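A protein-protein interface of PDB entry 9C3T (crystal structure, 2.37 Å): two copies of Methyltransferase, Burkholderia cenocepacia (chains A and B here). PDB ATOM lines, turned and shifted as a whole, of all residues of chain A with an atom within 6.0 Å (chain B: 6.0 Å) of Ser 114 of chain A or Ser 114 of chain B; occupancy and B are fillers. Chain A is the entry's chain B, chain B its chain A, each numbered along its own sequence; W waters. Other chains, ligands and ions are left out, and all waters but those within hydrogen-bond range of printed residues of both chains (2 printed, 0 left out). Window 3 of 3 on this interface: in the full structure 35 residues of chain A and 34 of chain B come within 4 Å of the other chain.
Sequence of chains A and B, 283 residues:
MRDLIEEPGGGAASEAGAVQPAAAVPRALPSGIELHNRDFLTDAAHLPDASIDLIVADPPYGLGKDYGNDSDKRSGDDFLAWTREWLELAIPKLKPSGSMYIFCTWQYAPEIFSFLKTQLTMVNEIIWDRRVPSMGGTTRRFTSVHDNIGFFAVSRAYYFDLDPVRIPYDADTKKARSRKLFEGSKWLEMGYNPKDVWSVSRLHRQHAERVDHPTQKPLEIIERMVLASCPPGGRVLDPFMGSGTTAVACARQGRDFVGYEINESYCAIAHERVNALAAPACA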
ATOM      1  N   ALA A 109     -26.007 -30.381  -6.127  1.00  0.00           N
ATOM      2  CA  ALA A 109     -26.236 -28.983  -5.712  1.00  0.00           C
ATOM      3  C   ALA A 109     -25.317 -28.025  -6.471  1.00  0.00           C
ATOM      4  O   ALA A 109     -25.841 -27.026  -6.974  1.00  0.00           O
ATOM      5  CB  ALA A 109     -26.082 -28.848  -4.226  1.00  0.00           C
ATOM      6  N   PRO A 110     -23.989 -28.240  -6.581  1.00  0.00           N
ATOM      7  CA  PRO A 110     -23.164 -27.312  -7.379  1.00  0.00           C
ATOM      8  C   PRO A 110     -23.699 -27.071  -8.778  1.00  0.00           C
ATOM      9  O   PRO A 110     -23.692 -25.928  -9.250  1.00  0.00           O
ATOM     10  CB  PRO A 110     -21.787 -27.998  -7.419  1.00  0.00           C
ATOM     11  CG  PRO A 110     -21.962 -29.337  -6.773  1.00  0.00           C
ATOM     12  CD  PRO A 110     -23.152 -29.234  -5.890  1.00  0.00           C
ATOM     13  N   GLU A 111     -24.163 -28.120  -9.460  1.00  0.00           N
ATOM     14  CA  GLU A 111     -24.698 -27.945 -10.807  1.00  0.00           C
ATOM     15  C   GLU A 111     -26.049 -27.243 -10.775  1.00  0.00           C
ATOM     16  O   GLU A 111     -26.301 -26.326 -11.565  1.00  0.00           O
ATOM     17  CB  GLU A 111     -24.813 -29.298 -11.511  1.00  0.00           C
ATOM     18  CG  GLU A 111     -23.523 -29.779 -12.153  1.00  0.00           C
ATOM     19  CD  GLU A 111     -22.476 -30.181 -11.133  1.00  0.00           C
ATOM     20  OE1 GLU A 111     -22.843 -30.413  -9.961  1.00  0.00           O
ATOM     21  OE2 GLU A 111     -21.286 -30.263 -11.502  1.00  0.00           O
ATOM     22  N   ILE A 112     -26.931 -27.661  -9.864  1.00  0.00           N
ATOM     23  CA  ILE A 112     -28.267 -27.073  -9.792  1.00  0.00           C
ATOM     24  C   ILE A 112     -28.179 -25.594  -9.436  1.00  0.00           C
ATOM     25  O   ILE A 112     -28.813 -24.743 -10.072  1.00  0.00           O
ATOM     26  CB  ILE A 112     -29.140 -27.843  -8.784  1.00  0.00           C
ATOM     27  CG1 ILE A 112     -29.490 -29.229  -9.325  1.00  0.00           C
ATOM     28  CG2 ILE A 112     -30.404 -27.059  -8.466  1.00  0.00           C
ATOM     29  CD1 ILE A 112     -29.990 -30.188  -8.266  1.00  0.00           C
ATOM     30  N   PHE A 113     -27.384 -25.265  -8.415  1.00  0.00           N
ATOM     31  CA  PHE A 113     -27.289 -23.877  -7.977  1.00  0.00           C
ATOM     32  C   PHE A 113     -26.613 -23.001  -9.023  1.00  0.00           C
ATOM     33  O   PHE A 113     -26.923 -21.810  -9.123  1.00  0.00           O
ATOM     34  CB  PHE A 113     -26.541 -23.790  -6.646  1.00  0.00           C
ATOM     35  CG  PHE A 113     -27.298 -24.371  -5.484  1.00  0.00           C
ATOM     36  CD1 PHE A 113     -28.612 -24.787  -5.631  1.00  0.00           C
ATOM     37  CD2 PHE A 113     -26.695 -24.500  -4.245  1.00  0.00           C
ATOM     38  CE1 PHE A 113     -29.309 -25.323  -4.567  1.00  0.00           C
ATOM     39  CE2 PHE A 113     -27.386 -25.036  -3.174  1.00  0.00           C
ATOM     40  CZ  PHE A 113     -28.695 -25.449  -3.336  1.00  0.00           C
ATOM     41  N   SER A 114     -25.700 -23.563  -9.795  1.00  0.00           N
ATOM     42  CA  SER A 114     -24.996 -22.780 -10.838  1.00  0.00           C
ATOM     43  C   SER A 114     -25.974 -22.385 -11.958  1.00  0.00           C
ATOM     44  O   SER A 114     -25.837 -21.277 -12.487  1.00  0.00           O
ATOM     45  CB  SER A 114     -23.788 -23.519 -11.343  1.00  0.00           C
ATOM     46  OG  SER A 114     -22.805 -23.625 -10.330  1.00  0.00           O
ATOM     47  N   PHE A 115     -26.946 -23.242 -12.266  1.00  0.00           N
ATOM     48  CA  PHE A 115     -27.934 -22.954 -13.337  1.00  0.00           C
ATOM     49  C   PHE A 115     -28.933 -21.927 -12.849  1.00  0.00           C
ATOM     50  O   PHE A 115     -29.341 -21.065 -13.627  1.00  0.00           O
ATOM     51  CB  PHE A 115     -28.664 -24.230 -13.767  1.00  0.00           C
ATOM     52  CG  PHE A 115     -29.990 -24.021 -14.483  1.00  0.00           C
ATOM     53  CD1 PHE A 115     -30.026 -23.654 -15.821  1.00  0.00           C
ATOM     54  CD2 PHE A 115     -31.196 -24.196 -13.818  1.00  0.00           C
ATOM     55  CE1 PHE A 115     -31.233 -23.461 -16.468  1.00  0.00           C
ATOM     56  CE2 PHE A 115     -32.399 -24.003 -14.471  1.00  0.00           C
ATOM     57  CZ  PHE A 115     -32.415 -23.637 -15.792  1.00  0.00           C
ATOM     58  N   LEU A 116     -29.319 -22.022 -11.586  1.00  0.00           N
ATOM     59  CA  LEU A 116     -30.369 -21.124 -11.060  1.00  0.00           C
ATOM     60  C   LEU A 116     -29.793 -19.713 -10.857  1.00  0.00           C
ATOM     61  O   LEU A 116     -30.569 -18.762 -10.963  1.00  0.00           O
ATOM     62  CB  LEU A 116     -30.968 -21.751  -9.806  1.00  0.00           C
ATOM     63  CG  LEU A 116     -31.863 -22.967 -10.044  1.00  0.00           C
ATOM     64  CD1 LEU A 116     -32.179 -23.656  -8.735  1.00  0.00           C
ATOM     65  CD2 LEU A 116     -33.128 -22.517 -10.737  1.00  0.00           C
ATOM     66  N   LYS A 117     -28.485 -19.588 -10.632  1.00  0.00           N
ATOM     67  CA  LYS A 117     -27.882 -18.262 -10.541  1.00  0.00           C
ATOM     68  C   LYS A 117     -27.877 -17.543 -11.882  1.00  0.00           C
ATOM     69  O   LYS A 117     -27.756 -16.314 -11.912  1.00  0.00           O
ATOM     70  CB  LYS A 117     -26.461 -18.363  -9.982  1.00  0.00           C
ATOM     71  CG  LYS A 117     -26.409 -18.855  -8.541  1.00  0.00           C
ATOM     72  CD  LYS A 117     -24.985 -19.083  -8.062  1.00  0.00           C
ATOM     73  CE  LYS A 117     -24.200 -17.784  -8.028  1.00  0.00           C
ATOM     74  NZ  LYS A 117     -22.977 -17.919  -7.192  1.00  0.00           N
ATOM     75  N   THR A 118     -28.013 -18.277 -12.988  1.00  0.00           N
ATOM     76  CA  THR A 118     -28.187 -17.655 -14.293  1.00  0.00           C
ATOM     77  C   THR A 118     -29.611 -17.165 -14.521  1.00  0.00           C
ATOM     78  O   THR A 118     -29.833 -16.338 -15.413  1.00  0.00           O
ATOM     79  CB  THR A 118     -27.804 -18.637 -15.404  1.00  0.00           C
ATOM     80  OG1 THR A 118     -28.740 -19.722 -15.426  1.00  0.00           O
ATOM     81  CG2 THR A 118     -26.406 -19.187 -15.166  1.00  0.00           C
ATOM     82  N   PHE A 152     -33.378 -18.742  -3.505  1.00  0.00           N
ATOM     83  CA  PHE A 152     -33.210 -17.849  -4.669  1.00  0.00           C
ATOM     84  C   PHE A 152     -34.375 -16.879  -4.733  1.00  0.00           C
ATOM     85  O   PHE A 152     -35.474 -17.201  -4.281  1.00  0.00           O
ATOM     86  CB  PHE A 152     -33.118 -18.698  -5.932  1.00  0.00           C
ATOM     87  CG  PHE A 152     -31.924 -19.630  -6.063  1.00  0.00           C
ATOM     88  CD1 PHE A 152     -31.965 -20.919  -5.549  1.00  0.00           C
ATOM     89  CD2 PHE A 152     -30.778 -19.224  -6.732  1.00  0.00           C
ATOM     90  CE1 PHE A 152     -30.882 -21.766  -5.685  1.00  0.00           C
ATOM     91  CE2 PHE A 152     -29.699 -20.078  -6.867  1.00  0.00           C
ATOM     92  CZ  PHE A 152     -29.753 -21.343  -6.340  1.00  0.00           C
ATOM     93  N   ALA B 109     -19.199 -21.346  -4.100  1.00  0.00           N
ATOM     94  CA  ALA B 109     -19.066 -22.800  -4.017  1.00  0.00           C
ATOM     95  C   ALA B 109     -19.664 -23.534  -5.213  1.00  0.00           C
ATOM     96  O   ALA B 109     -18.966 -24.387  -5.790  1.00  0.00           O
ATOM     97  CB  ALA B 109     -19.680 -23.292  -2.703  1.00  0.00           C
ATOM     98  N   PRO B 110     -20.914 -23.282  -5.632  1.00  0.00           N
ATOM     99  CA  PRO B 110     -21.483 -24.103  -6.719  1.00  0.00           C
ATOM    100  C   PRO B 110     -20.670 -24.069  -7.998  1.00  0.00           C
ATOM    101  O   PRO B 110     -20.552 -25.096  -8.677  1.00  0.00           O
ATOM    102  CB  PRO B 110     -22.881 -23.502  -6.927  1.00  0.00           C
ATOM    103  CG  PRO B 110     -22.842 -22.164  -6.286  1.00  0.00           C
ATOM    104  CD  PRO B 110     -21.873 -22.266  -5.162  1.00  0.00           C
ATOM    105  N   GLU B 111     -20.101 -22.915  -8.349  1.00  0.00           N
ATOM    106  CA  GLU B 111     -19.286 -22.831  -9.554  1.00  0.00           C
ATOM    107  C   GLU B 111     -17.914 -23.462  -9.352  1.00  0.00           C
ATOM    108  O   GLU B 111     -17.416 -24.160 -10.241  1.00  0.00           O
ATOM    109  CB  GLU B 111     -19.143 -21.374  -9.990  1.00  0.00           C
ATOM    110  CG  GLU B 111     -20.391 -20.793 -10.627  1.00  0.00           C
ATOM    111  CD  GLU B 111     -21.294 -20.118  -9.617  1.00  0.00           C
ATOM    112  OE1 GLU B 111     -20.984 -20.172  -8.409  1.00  0.00           O
ATOM    113  OE2 GLU B 111     -22.315 -19.531 -10.032  1.00  0.00           O
ATOM    114  N   ILE B 112     -17.288 -23.221  -8.198  1.00  0.00           N
ATOM    115  CA  ILE B 112     -15.979 -23.813  -7.924  1.00  0.00           C
ATOM    116  C   ILE B 112     -16.078 -25.332  -7.919  1.00  0.00           C
ATOM    117  O   ILE B 112     -15.268 -26.029  -8.542  1.00  0.00           O
ATOM    118  CB  ILE B 112     -15.412 -23.282  -6.594  1.00  0.00           C
ATOM    119  CG1 ILE B 112     -14.932 -21.837  -6.751  1.00  0.00           C
ATOM    120  CG2 ILE B 112     -14.280 -24.175  -6.105  1.00  0.00           C
ATOM    121  CD1 ILE B 112     -14.712 -21.120  -5.434  1.00  0.00           C
ATOM    122  N   PHE B 113     -17.081 -25.867  -7.219  1.00  0.00           N
ATOM    123  CA  PHE B 113     -17.260 -27.314  -7.162  1.00  0.00           C
ATOM    124  C   PHE B 113     -17.650 -27.885  -8.519  1.00  0.00           C
ATOM    125  O   PHE B 113     -17.260 -29.010  -8.850  1.00  0.00           O
ATOM    126  CB  PHE B 113     -18.311 -27.675  -6.112  1.00  0.00           C
ATOM    127  CG  PHE B 113     -17.915 -27.327  -4.703  1.00  0.00           C
ATOM    128  CD1 PHE B 113     -16.604 -26.992  -4.393  1.00  0.00           C
ATOM    129  CD2 PHE B 113     -18.854 -27.338  -3.684  1.00  0.00           C
ATOM    130  CE1 PHE B 113     -16.240 -26.675  -3.098  1.00  0.00           C
ATOM    131  CE2 PHE B 113     -18.496 -27.022  -2.386  1.00  0.00           C
ATOM    132  CZ  PHE B 113     -17.187 -26.689  -2.093  1.00  0.00           C
ATOM    133  N   SER B 114     -18.381 -27.127  -9.320  1.00  0.00           N
ATOM    134  CA  SER B 114     -18.775 -27.608 -10.663  1.00  0.00           C
ATOM    135  C   SER B 114     -17.533 -27.768 -11.548  1.00  0.00           C
ATOM    136  O   SER B 114     -17.477 -28.743 -12.306  1.00  0.00           O
ATOM    137  CB  SER B 114     -19.806 -26.715 -11.281  1.00  0.00           C
ATOM    138  OG  SER B 114     -21.018 -26.756 -10.548  1.00  0.00           O
ATOM    139  N   PHE B 115     -16.561 -26.863 -11.414  1.00  0.00           N
ATOM    140  CA  PHE B 115     -15.311 -26.936 -12.216  1.00  0.00           C
ATOM    141  C   PHE B 115     -14.446 -28.072 -11.713  1.00  0.00           C
ATOM    142  O   PHE B 115     -13.855 -28.793 -12.520  1.00  0.00           O
ATOM    143  CB  PHE B 115     -14.522 -25.627 -12.133  1.00  0.00           C
ATOM    144  CG  PHE B 115     -13.028 -25.766 -12.383  1.00  0.00           C
ATOM    145  CD1 PHE B 115     -12.539 -25.995 -13.663  1.00  0.00           C
ATOM    146  CD2 PHE B 115     -12.120 -25.670 -11.337  1.00  0.00           C
ATOM    147  CE1 PHE B 115     -11.181 -26.128 -13.887  1.00  0.00           C
ATOM    148  CE2 PHE B 115     -10.764 -25.804 -11.570  1.00  0.00           C
ATOM    149  CZ  PHE B 115     -10.298 -26.030 -12.842  1.00  0.00           C
ATOM    150  N   LEU B 116     -14.369 -28.223 -10.404  1.00  0.00           N
ATOM    151  CA  LEU B 116     -13.463 -29.237  -9.832  1.00  0.00           C
ATOM    152  C   LEU B 116     -14.034 -30.644 -10.069  1.00  0.00           C
ATOM    153  O   LEU B 116     -13.258 -31.592 -10.020  1.00  0.00           O
ATOM    154  CB  LEU B 116     -13.250 -28.895  -8.361  1.00  0.00           C
ATOM    155  CG  LEU B 116     -12.160 -27.867  -8.069  1.00  0.00           C
ATOM    156  CD1 LEU B 116     -12.033 -27.658  -6.577  1.00  0.00           C
ATOM    157  CD2 LEU B 116     -10.864 -28.388  -8.650  1.00  0.00           C
ATOM    158  N   LYS B 117     -15.323 -30.753 -10.370  1.00  0.00           N
ATOM    159  CA  LYS B 117     -15.940 -32.069 -10.676  1.00  0.00           C
ATOM    160  C   LYS B 117     -15.532 -32.503 -12.091  1.00  0.00           C
ATOM    161  O   LYS B 117     -15.598 -33.711 -12.365  1.00  0.00           O
ATOM    162  CB  LYS B 117     -17.455 -32.038 -10.452  1.00  0.00           C
ATOM    163  CG  LYS B 117     -17.891 -32.315  -9.023  1.00  0.00           C
ATOM    164  CD  LYS B 117     -19.352 -31.971  -8.772  1.00  0.00           C
ATOM    165  CE  LYS B 117     -20.260 -33.040  -9.279  1.00  0.00           C
ATOM    166  NZ  LYS B 117     -21.670 -32.666  -9.182  1.00  0.00           N
ATOM    167  N   THR B 118     -15.144 -31.570 -12.955  1.00  0.00           N
ATOM    168  CA  THR B 118     -14.619 -31.921 -14.268  1.00  0.00           C
ATOM    169  C   THR B 118     -13.138 -32.272 -14.233  1.00  0.00           C
ATOM    170  O   THR B 118     -12.624 -32.818 -15.215  1.00  0.00           O
ATOM    171  CB  THR B 118     -14.841 -30.773 -15.254  1.00  0.00           C
ATOM    172  OG1 THR B 118     -14.052 -29.643 -14.859  1.00  0.00           O
ATOM    173  CG2 THR B 118     -16.310 -30.379 -15.293  1.00  0.00           C
ATOM    174  N   PHE B 152     -12.375 -33.514  -2.574  1.00  0.00           N
ATOM    175  CA  PHE B 152     -12.228 -34.113  -3.921  1.00  0.00           C
ATOM    176  C   PHE B 152     -11.095 -35.138  -3.934  1.00  0.00           C
ATOM    177  O   PHE B 152     -10.203 -35.071  -3.084  1.00  0.00           O
ATOM    178  CB  PHE B 152     -12.003 -32.980  -4.920  1.00  0.00           C
ATOM    179  CG  PHE B 152     -13.124 -31.968  -5.092  1.00  0.00           C
ATOM    180  CD1 PHE B 152     -13.211 -30.852  -4.272  1.00  0.00           C
ATOM    181  CD2 PHE B 152     -14.065 -32.118  -6.101  1.00  0.00           C
ATOM    182  CE1 PHE B 152     -14.225 -29.929  -4.441  1.00  0.00           C
ATOM    183  CE2 PHE B 152     -15.073 -31.186  -6.267  1.00  0.00           C
ATOM    184  CZ  PHE B 152     -15.152 -30.098  -5.435  1.00  0.00           C
HETATM  185  O   HOH W   1     -23.427 -19.742 -12.693  1.00  0.00           O
HETATM  186  O   HOH W   2     -19.702 -30.817 -13.672  1.00  0.00           O
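Along chain A the printed residues that touch a printed residue of chain B span positions 110 to 117.
Printed residues of chain B that touch a printed residue of chain A: Pro 110, Glu 111, Phe 113, Ser 114 and Lys 117.
Hydrophobic or aromatic side chains of chain B that line the printed part of chain A: Pro 110 and Phe 113.
Among the printed residues, 10 pairs touch across the chains.
Water W2 lies within hydrogen-bond range of OE2 of Glu 111 of chain A (2.7 Å) and O of Ser 114 of chain B (3.3 Å).
Water W1 lies within hydrogen-bond range of the backbone carbonyl oxygen of Ser 114 of chain A (2.9 Å) and the side-chain carboxylate of Glu 111 of chain B (2.9 Å).
The backbone carbonyl oxygen of Pro 110 of chain B is in hydrogen-bond range of the side-chain hydroxyl of Ser 114 of chain B, at 2.5 Å.
O of Pro 110 of chain A is in hydrogen-bond range of OG of Ser 114 of chain A (2.7 Å).
The side-chain hydroxyl (OG) of Ser 114 of chain A is in hydrogen-bond range of the backbone NH (N) of Glu 111 of chain B, 3.4 Å away.
The backbone carbonyl oxygen (O) of Pro 110 of chain A sits at hydrogen-bond distance from the side-chain hydroxyl (OG) of Ser 114 of chain B.
OG of Ser 114 of chain A sits at hydrogen-bond distance from O of Pro 110 of chain B, 3.2 Å away.
NZ of Lys 117 of chain B is in salt-bridge range of OE1 of Glu 111 of chain A, 2.7 Å away.
The backbone carbonyl oxygen of Pro 110 of chain B sits close to the backbone carbonyl oxygen of Pro 110 of chain A, at 3.3 Å.
OE1 of Glu 111 of chain B is in salt-bridge range of NZ of Lys 117 of chain A, 3.2 Å away.
Printed residues of chain B within 4 Å of Glu 111 of chain A: Ser 114 (3.6 Å) and Lys 117 (2.7 Å).
Of the printed residues of chain B, Phe 113 of chain A touches Pro 110.
Of chain B, only Pro 110 (3.2 Å), Glu 111 (3.4 Å) and Ser 114 (3.6 Å) come within 4 Å of Ser 114 of chain A.
Printed residues of chain B within 4 Å of Lys 117 of chain A: Glu 111.
Printed residues of chain A within 4 Å of Glu 111 of chain B: Ser 114 (3.4 Å) and Lys 117 (3.2 Å).
Of chain A, only Pro 110 (3.1 Å), Glu 111 (3.6 Å) and Ser 114 (3.6 Å) come within 4 Å of Ser 114 of chain B.
The nearest printed residue of chain A that does not touch Ser 114 of chain B is Ala 109 of chain A (6.0 Å).
Among the printed residues, pairs that only touch across the chains: Pro 110 of chain A with Phe 113 of chain B (3.7 Å), Glu 111 of chain A with Ser 114 of chain B (3.6 Å), Phe 113 of chain A with Pro 110 of chain B (3.7 Å) and Ser 114 of chain A with Ser 114 of chain B (3.6 Å).
Pro 110 of chain A touches Phe 113 of chain B, and with the chains exchanged Phe 113 of chain A touches Pro 110 of chain B.
Glu 111 of chain A touches Ser 114 of chain B, and with the chains exchanged Ser 114 of chain A touches Glu 111 of chain B.
Glu 111 of chain A touches Lys 117 of chain B, and with the chains exchanged Lys 117 of chain A touches Glu 111 of chain B.
Ser 114 of chain A touches its own counterpart, Ser 114 of chain B.
11 positions are printed for both chains.
Of the 10 pairs that touch across the chains among the printed residues, 10 have their exchanged pair printed and touching as well.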
